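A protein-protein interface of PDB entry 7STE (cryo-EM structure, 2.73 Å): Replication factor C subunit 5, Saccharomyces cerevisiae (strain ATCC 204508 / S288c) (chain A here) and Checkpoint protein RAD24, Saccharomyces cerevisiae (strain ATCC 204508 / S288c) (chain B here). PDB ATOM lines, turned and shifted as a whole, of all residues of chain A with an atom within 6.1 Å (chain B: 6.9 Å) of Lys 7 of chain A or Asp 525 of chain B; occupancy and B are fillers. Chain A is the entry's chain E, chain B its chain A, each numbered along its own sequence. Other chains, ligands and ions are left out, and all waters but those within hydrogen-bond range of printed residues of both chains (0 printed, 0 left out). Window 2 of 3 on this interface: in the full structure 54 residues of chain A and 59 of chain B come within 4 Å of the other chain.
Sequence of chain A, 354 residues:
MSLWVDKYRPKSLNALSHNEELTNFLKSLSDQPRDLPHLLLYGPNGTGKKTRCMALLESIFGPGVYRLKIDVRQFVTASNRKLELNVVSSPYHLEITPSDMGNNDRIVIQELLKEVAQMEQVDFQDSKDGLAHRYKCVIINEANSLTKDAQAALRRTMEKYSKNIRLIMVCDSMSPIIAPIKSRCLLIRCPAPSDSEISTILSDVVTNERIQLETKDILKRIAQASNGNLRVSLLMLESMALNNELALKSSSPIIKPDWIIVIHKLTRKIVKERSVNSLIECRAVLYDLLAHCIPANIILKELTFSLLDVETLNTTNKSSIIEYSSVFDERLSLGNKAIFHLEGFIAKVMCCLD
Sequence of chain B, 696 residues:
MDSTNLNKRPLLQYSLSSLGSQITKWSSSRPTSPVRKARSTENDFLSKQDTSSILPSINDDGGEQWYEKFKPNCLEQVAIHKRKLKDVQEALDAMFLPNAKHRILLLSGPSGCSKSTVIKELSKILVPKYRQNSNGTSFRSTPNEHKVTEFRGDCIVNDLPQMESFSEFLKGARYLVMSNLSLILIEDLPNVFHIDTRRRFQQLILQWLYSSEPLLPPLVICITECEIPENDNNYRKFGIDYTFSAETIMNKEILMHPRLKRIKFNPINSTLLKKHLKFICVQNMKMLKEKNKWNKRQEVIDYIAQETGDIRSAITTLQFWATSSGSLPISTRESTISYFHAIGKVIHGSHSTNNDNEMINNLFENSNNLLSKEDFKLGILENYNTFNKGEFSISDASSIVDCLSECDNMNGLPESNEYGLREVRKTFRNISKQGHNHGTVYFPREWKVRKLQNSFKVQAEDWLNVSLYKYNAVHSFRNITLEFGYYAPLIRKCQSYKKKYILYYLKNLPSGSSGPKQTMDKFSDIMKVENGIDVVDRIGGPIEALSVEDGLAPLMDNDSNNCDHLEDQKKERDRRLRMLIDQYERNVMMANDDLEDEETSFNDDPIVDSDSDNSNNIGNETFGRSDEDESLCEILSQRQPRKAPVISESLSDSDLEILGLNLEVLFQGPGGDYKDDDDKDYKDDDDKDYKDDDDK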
ATOM      1  N   MET A   1     -16.011  23.499 -15.452  1.00  0.00           N
ATOM      2  CA  MET A   1     -16.630  24.296 -14.355  1.00  0.00           C
ATOM      3  C   MET A   1     -15.569  25.105 -13.616  1.00  0.00           C
ATOM      4  O   MET A   1     -14.467  25.311 -14.123  1.00  0.00           O
ATOM      5  CB  MET A   1     -17.368  23.379 -13.378  1.00  0.00           C
ATOM      6  N   SER A   2     -15.908  25.562 -12.413  1.00  0.00           N
ATOM      7  CA  SER A   2     -14.967  26.334 -11.617  1.00  0.00           C
ATOM      8  C   SER A   2     -13.750  25.488 -11.260  1.00  0.00           C
ATOM      9  O   SER A   2     -13.848  24.278 -11.037  1.00  0.00           O
ATOM     10  CB  SER A   2     -15.641  26.846 -10.343  1.00  0.00           C
ATOM     11  OG  SER A   2     -14.727  27.568  -9.537  1.00  0.00           O
ATOM     12  N   LEU A   3     -12.592  26.139 -11.210  1.00  0.00           N
ATOM     13  CA  LEU A   3     -11.358  25.443 -10.875  1.00  0.00           C
ATOM     14  C   LEU A   3     -11.447  24.852  -9.473  1.00  0.00           C
ATOM     15  O   LEU A   3     -12.064  25.422  -8.571  1.00  0.00           O
ATOM     16  CB  LEU A   3     -10.166  26.396 -10.967  1.00  0.00           C
ATOM     17  CG  LEU A   3      -9.825  26.930 -12.359  1.00  0.00           C
ATOM     18  CD1 LEU A   3      -8.722  27.972 -12.272  1.00  0.00           C
ATOM     19  CD2 LEU A   3      -9.423  25.800 -13.294  1.00  0.00           C
ATOM     20  N   TRP A   4     -10.816  23.687  -9.296  1.00  0.00           N
ATOM     21  CA  TRP A   4     -10.838  23.029  -7.994  1.00  0.00           C
ATOM     22  C   TRP A   4     -10.270  23.929  -6.907  1.00  0.00           C
ATOM     23  O   TRP A   4     -10.617  23.777  -5.730  1.00  0.00           O
ATOM     24  CB  TRP A   4     -10.054  21.717  -8.054  1.00  0.00           C
ATOM     25  CG  TRP A   4     -10.637  20.702  -8.992  1.00  0.00           C
ATOM     26  CD1 TRP A   4     -11.793  20.814  -9.708  1.00  0.00           C
ATOM     27  CD2 TRP A   4     -10.087  19.419  -9.314  1.00  0.00           C
ATOM     28  NE1 TRP A   4     -11.997  19.680 -10.456  1.00  0.00           N
ATOM     29  CE2 TRP A   4     -10.964  18.809 -10.232  1.00  0.00           C
ATOM     30  CE3 TRP A   4      -8.940  18.728  -8.915  1.00  0.00           C
ATOM     31  CZ2 TRP A   4     -10.730  17.540 -10.757  1.00  0.00           C
ATOM     32  CZ3 TRP A   4      -8.708  17.469  -9.438  1.00  0.00           C
ATOM     33  CH2 TRP A   4      -9.599  16.888 -10.348  1.00  0.00           C
ATOM     34  N   VAL A   5      -9.397  24.868  -7.277  1.00  0.00           N
ATOM     35  CA  VAL A   5      -8.844  25.796  -6.294  1.00  0.00           C
ATOM     36  C   VAL A   5      -9.950  26.655  -5.693  1.00  0.00           C
ATOM     37  O   VAL A   5      -9.971  26.905  -4.481  1.00  0.00           O
ATOM     38  CB  VAL A   5      -7.739  26.654  -6.940  1.00  0.00           C
ATOM     39  CG1 VAL A   5      -8.315  27.558  -8.020  1.00  0.00           C
ATOM     40  CG2 VAL A   5      -7.016  27.473  -5.888  1.00  0.00           C
ATOM     41  N   ASP A   6     -10.883  27.119  -6.525  1.00  0.00           N
ATOM     42  CA  ASP A   6     -11.998  27.929  -6.048  1.00  0.00           C
ATOM     43  C   ASP A   6     -13.247  27.106  -5.763  1.00  0.00           C
ATOM     44  O   ASP A   6     -14.080  27.523  -4.950  1.00  0.00           O
ATOM     45  CB  ASP A   6     -12.341  29.015  -7.072  1.00  0.00           C
ATOM     46  CG  ASP A   6     -11.115  29.737  -7.591  1.00  0.00           C
ATOM     47  OD1 ASP A   6     -10.643  29.391  -8.695  1.00  0.00           O
ATOM     48  OD2 ASP A   6     -10.623  30.650  -6.896  1.00  0.00           O
ATOM     49  N   LYS A   7     -13.398  25.950  -6.412  1.00  0.00           N
ATOM     50  CA  LYS A   7     -14.604  25.149  -6.225  1.00  0.00           C
ATOM     51  C   LYS A   7     -14.738  24.677  -4.783  1.00  0.00           C
ATOM     52  O   LYS A   7     -15.834  24.709  -4.211  1.00  0.00           O
ATOM     53  CB  LYS A   7     -14.590  23.955  -7.180  1.00  0.00           C
ATOM     54  CG  LYS A   7     -15.779  23.019  -7.024  1.00  0.00           C
ATOM     55  CD  LYS A   7     -15.794  21.958  -8.112  1.00  0.00           C
ATOM     56  CE  LYS A   7     -16.993  21.036  -7.973  1.00  0.00           C
ATOM     57  NZ  LYS A   7     -17.147  20.137  -9.149  1.00  0.00           N
ATOM     58  N   TYR A   8     -13.635  24.238  -4.178  1.00  0.00           N
ATOM     59  CA  TYR A   8     -13.637  23.707  -2.821  1.00  0.00           C
ATOM     60  C   TYR A   8     -13.110  24.711  -1.802  1.00  0.00           C
ATOM     61  O   TYR A   8     -12.751  24.321  -0.686  1.00  0.00           O
ATOM     62  CB  TYR A   8     -12.820  22.416  -2.764  1.00  0.00           C
ATOM     63  CG  TYR A   8     -13.371  21.317  -3.642  1.00  0.00           C
ATOM     64  CD1 TYR A   8     -14.436  20.534  -3.219  1.00  0.00           C
ATOM     65  CD2 TYR A   8     -12.831  21.066  -4.896  1.00  0.00           C
ATOM     66  CE1 TYR A   8     -14.946  19.529  -4.018  1.00  0.00           C
ATOM     67  CE2 TYR A   8     -13.334  20.064  -5.702  1.00  0.00           C
ATOM     68  CZ  TYR A   8     -14.392  19.299  -5.258  1.00  0.00           C
ATOM     69  OH  TYR A   8     -14.898  18.299  -6.057  1.00  0.00           O
ATOM     70  N   ARG A   9     -13.054  25.987  -2.161  1.00  0.00           N
ATOM     71  CA  ARG A   9     -12.594  27.001  -1.222  1.00  0.00           C
ATOM     72  C   ARG A   9     -13.565  27.092  -0.049  1.00  0.00           C
ATOM     73  O   ARG A   9     -14.777  27.200  -0.266  1.00  0.00           O
ATOM     74  CB  ARG A   9     -12.478  28.356  -1.918  1.00  0.00           C
ATOM     75  CG  ARG A   9     -12.214  29.516  -0.971  1.00  0.00           C
ATOM     76  CD  ARG A   9     -11.400  30.608  -1.644  1.00  0.00           C
ATOM     77  NE  ARG A   9     -11.686  31.926  -1.088  1.00  0.00           N
ATOM     78  CZ  ARG A   9     -10.863  32.964  -1.153  1.00  0.00           C
ATOM     79  NH1 ARG A   9      -9.686  32.880  -1.750  1.00  0.00           N
ATOM     80  NH2 ARG A   9     -11.232  34.118  -0.605  1.00  0.00           N
ATOM     81  N   GLU A 209     -13.767  14.270  -6.222  1.00  0.00           N
ATOM     82  CA  GLU A 209     -13.625  14.322  -7.671  1.00  0.00           C
ATOM     83  C   GLU A 209     -13.479  12.949  -8.312  1.00  0.00           C
ATOM     84  O   GLU A 209     -13.453  12.859  -9.545  1.00  0.00           O
ATOM     85  CB  GLU A 209     -12.418  15.190  -8.048  1.00  0.00           C
ATOM     86  CG  GLU A 209     -12.668  16.683  -7.919  1.00  0.00           C
ATOM     87  CD  GLU A 209     -13.606  17.215  -8.984  1.00  0.00           C
ATOM     88  OE1 GLU A 209     -13.851  16.496  -9.976  1.00  0.00           O
ATOM     89  OE2 GLU A 209     -14.099  18.352  -8.830  1.00  0.00           O
ATOM     90  N   ARG B 492      -7.684  24.736 -18.901  1.00  0.00           N
ATOM     91  CA  ARG B 492      -8.766  25.051 -19.828  1.00  0.00           C
ATOM     92  C   ARG B 492      -8.532  24.408 -21.189  1.00  0.00           C
ATOM     93  O   ARG B 492      -9.478  23.927 -21.820  1.00  0.00           O
ATOM     94  CB  ARG B 492      -8.917  26.566 -19.964  1.00  0.00           C
ATOM     95  CG  ARG B 492      -9.320  27.269 -18.673  1.00  0.00           C
ATOM     96  CD  ARG B 492     -10.713  26.865 -18.212  1.00  0.00           C
ATOM     97  NE  ARG B 492     -11.060  27.465 -16.928  1.00  0.00           N
ATOM     98  CZ  ARG B 492     -12.063  27.064 -16.159  1.00  0.00           C
ATOM     99  NH1 ARG B 492     -12.848  26.059 -16.513  1.00  0.00           N
ATOM    100  NH2 ARG B 492     -12.284  27.686 -15.004  1.00  0.00           N
ATOM    101  N   GLN B 495      -9.384  20.731 -20.847  1.00  0.00           N
ATOM    102  CA  GLN B 495     -10.829  20.549 -20.755  1.00  0.00           C
ATOM    103  C   GLN B 495     -11.496  20.759 -22.108  1.00  0.00           C
ATOM    104  O   GLN B 495     -12.410  20.014 -22.480  1.00  0.00           O
ATOM    105  CB  GLN B 495     -11.409  21.504 -19.713  1.00  0.00           C
ATOM    106  CG  GLN B 495     -11.094  21.112 -18.278  1.00  0.00           C
ATOM    107  CD  GLN B 495     -11.461  22.194 -17.282  1.00  0.00           C
ATOM    108  OE1 GLN B 495     -11.726  23.336 -17.656  1.00  0.00           O
ATOM    109  NE2 GLN B 495     -11.478  21.838 -16.003  1.00  0.00           N
ATOM    110  N   ASP B 521     -21.896  11.371 -15.659  1.00  0.00           N
ATOM    111  CA  ASP B 521     -21.497  12.770 -15.571  1.00  0.00           C
ATOM    112  C   ASP B 521     -20.049  12.893 -15.108  1.00  0.00           C
ATOM    113  O   ASP B 521     -19.697  13.819 -14.379  1.00  0.00           O
ATOM    114  CB  ASP B 521     -22.420  13.531 -14.617  1.00  0.00           C
ATOM    115  N   LYS B 522     -19.212  11.946 -15.538  1.00  0.00           N
ATOM    116  CA  LYS B 522     -17.804  11.979 -15.156  1.00  0.00           C
ATOM    117  C   LYS B 522     -17.118  13.229 -15.692  1.00  0.00           C
ATOM    118  O   LYS B 522     -16.323  13.861 -14.987  1.00  0.00           O
ATOM    119  CB  LYS B 522     -17.097  10.721 -15.660  1.00  0.00           C
ATOM    120  CG  LYS B 522     -15.608  10.682 -15.359  1.00  0.00           C
ATOM    121  CD  LYS B 522     -15.035   9.289 -15.573  1.00  0.00           C
ATOM    122  CE  LYS B 522     -13.529   9.270 -15.377  1.00  0.00           C
ATOM    123  NZ  LYS B 522     -12.965   7.897 -15.490  1.00  0.00           N
ATOM    124  N   PHE B 523     -17.414  13.601 -16.937  1.00  0.00           N
ATOM    125  CA  PHE B 523     -16.834  14.778 -17.574  1.00  0.00           C
ATOM    126  C   PHE B 523     -17.876  15.873 -17.788  1.00  0.00           C
ATOM    127  O   PHE B 523     -17.736  16.703 -18.689  1.00  0.00           O
ATOM    128  CB  PHE B 523     -16.185  14.396 -18.903  1.00  0.00           C
ATOM    129  CG  PHE B 523     -15.410  13.110 -18.852  1.00  0.00           C
ATOM    130  CD1 PHE B 523     -14.105  13.089 -18.389  1.00  0.00           C
ATOM    131  CD2 PHE B 523     -15.986  11.923 -19.269  1.00  0.00           C
ATOM    132  CE1 PHE B 523     -13.391  11.907 -18.342  1.00  0.00           C
ATOM    133  CE2 PHE B 523     -15.276  10.738 -19.224  1.00  0.00           C
ATOM    134  CZ  PHE B 523     -13.977  10.730 -18.761  1.00  0.00           C
ATOM    135  N   SER B 524     -18.928  15.884 -16.965  1.00  0.00           N
ATOM    136  CA  SER B 524     -19.989  16.870 -17.139  1.00  0.00           C
ATOM    137  C   SER B 524     -19.458  18.289 -16.974  1.00  0.00           C
ATOM    138  O   SER B 524     -19.795  19.182 -17.759  1.00  0.00           O
ATOM    139  CB  SER B 524     -21.118  16.603 -16.143  1.00  0.00           C
ATOM    140  OG  SER B 524     -20.644  16.653 -14.809  1.00  0.00           O
ATOM    141  N   ASP B 525     -18.630  18.519 -15.952  1.00  0.00           N
ATOM    142  CA  ASP B 525     -18.057  19.845 -15.759  1.00  0.00           C
ATOM    143  C   ASP B 525     -17.044  20.182 -16.846  1.00  0.00           C
ATOM    144  O   ASP B 525     -16.869  21.357 -17.185  1.00  0.00           O
ATOM    145  CB  ASP B 525     -17.401  19.937 -14.381  1.00  0.00           C
ATOM    146  CG  ASP B 525     -18.412  19.903 -13.252  1.00  0.00           C
ATOM    147  OD1 ASP B 525     -19.616  19.732 -13.536  1.00  0.00           O
ATOM    148  OD2 ASP B 525     -18.001  20.048 -12.081  1.00  0.00           O
ATOM    149  N   ILE B 526     -16.372  19.171 -17.400  1.00  0.00           N
ATOM    150  CA  ILE B 526     -15.350  19.423 -18.412  1.00  0.00           C
ATOM    151  C   ILE B 526     -15.974  20.031 -19.662  1.00  0.00           C
ATOM    152  O   ILE B 526     -15.445  20.994 -20.231  1.00  0.00           O
ATOM    153  CB  ILE B 526     -14.585  18.125 -18.729  1.00  0.00           C
ATOM    154  CG1 ILE B 526     -13.961  17.564 -17.446  1.00  0.00           C
ATOM    155  CG2 ILE B 526     -13.514  18.377 -19.787  1.00  0.00           C
ATOM    156  CD1 ILE B 526     -12.939  16.471 -17.672  1.00  0.00           C
ATOM    157  N   MET B 527     -17.104  19.483 -20.113  1.00  0.00           N
ATOM    158  CA  MET B 527     -17.735  19.987 -21.328  1.00  0.00           C
ATOM    159  C   MET B 527     -18.385  21.350 -21.129  1.00  0.00           C
ATOM    160  O   MET B 527     -18.780  21.975 -22.119  1.00  0.00           O
ATOM    161  CB  MET B 527     -18.778  18.990 -21.839  1.00  0.00           C
ATOM    162  CG  MET B 527     -19.974  18.790 -20.921  1.00  0.00           C
ATOM    163  SD  MET B 527     -21.128  17.565 -21.569  1.00  0.00           S
ATOM    164  CE  MET B 527     -22.378  17.552 -20.288  1.00  0.00           C
ATOM    165  N   LYS B 528     -18.505  21.822 -19.887  1.00  0.00           N
ATOM    166  CA  LYS B 528     -19.070  23.141 -19.633  1.00  0.00           C
ATOM    167  C   LYS B 528     -18.156  24.270 -20.089  1.00  0.00           C
ATOM    168  O   LYS B 528     -18.607  25.418 -20.158  1.00  0.00           O
ATOM    169  CB  LYS B 528     -19.372  23.296 -18.140  1.00  0.00           C
ATOM    170  CG  LYS B 528     -20.256  24.488 -17.802  1.00  0.00           C
ATOM    171  CD  LYS B 528     -20.501  24.593 -16.306  1.00  0.00           C
ATOM    172  CE  LYS B 528     -21.497  23.549 -15.827  1.00  0.00           C
ATOM    173  NZ  LYS B 528     -21.818  23.706 -14.382  1.00  0.00           N
ATOM    174  N   VAL B 529     -16.894  23.976 -20.405  1.00  0.00           N
ATOM    175  CA  VAL B 529     -15.965  25.018 -20.822  1.00  0.00           C
ATOM    176  C   VAL B 529     -16.441  25.607 -22.142  1.00  0.00           C
ATOM    177  O   VAL B 529     -16.676  24.880 -23.115  1.00  0.00           O
ATOM    178  CB  VAL B 529     -14.544  24.456 -20.937  1.00  0.00           C
ATOM    179  CG1 VAL B 529     -13.591  25.505 -21.496  1.00  0.00           C
ATOM    180  CG2 VAL B 529     -14.060  23.961 -19.582  1.00  0.00           C
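N of Met 1 of chain A lies within hydrogen-bond range of O of Asp 525 of chain B, 2.9 Å away.
The side-chain amino group (NZ) of Lys 7 of chain A is in salt-bridge range of the side-chain carboxylate (OD2) of Asp 525 of chain B (3.1 Å).
O of Met 1 of chain A is in hydrogen-bond range of NH1 of Arg 492 of chain B (3.0 Å).
Of the 11 printed residues of chain B, 2 touch a printed residue of chain A.
Printed residues of chain A that touch a printed residue of chain B: Met 1, Leu 3 and Lys 7.
Hydrophobic or aromatic side chains of chain A that line the printed part of chain B: Met 1 and Leu 3.
Along chain A the printed residues that touch a printed residue of chain B span positions 1 to 7.
The side-chain amino group (NZ) of Lys 7 of chain A lies within salt-bridge range of the side-chain carboxylate (OE2) of Glu 209 of chain A (3.5 Å).
The guanidinium group of Arg 492 of chain B sits at hydrogen-bond distance from the side-chain amide oxygen of Gln 495 of chain B (3.2 Å).
The side-chain hydroxyl (OG) of Ser 524 of chain B lies within hydrogen-bond range of the side-chain carboxylate (OD1) of Asp 525 of chain B (3.5 Å).
Printed residues of chain B within 4 Å of Met 1 of chain A: Arg 492 (3.0 Å) and Asp 525 (2.9 Å).
Of the printed residues of chain B, Leu 3 of chain A touches Arg 492.
Of the printed residues of chain A, Arg 492 of chain B touches Met 1 and Leu 3.
Ser 524 of chain B touches none of the printed residues of chain A.
Of chain A, only Met 1 (2.9 Å) and Lys 7 (3.1 Å) come within 4 Å of Asp 525 of chain B.
Ile 526 of chain B touches none of the printed residues of chain A.
The nearest printed residue of chain B that does not touch Lys 7 of chain A is Ser 524 of chain B (7.5 Å).
The nearest residue of chain A that does not touch Asp 525 of chain B is Glu 209 of chain A (5.4 Å).
Among the printed residues, pairs that only touch across the chains: Leu 3 of chain A with Arg 492 of chain B (3.7 Å).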
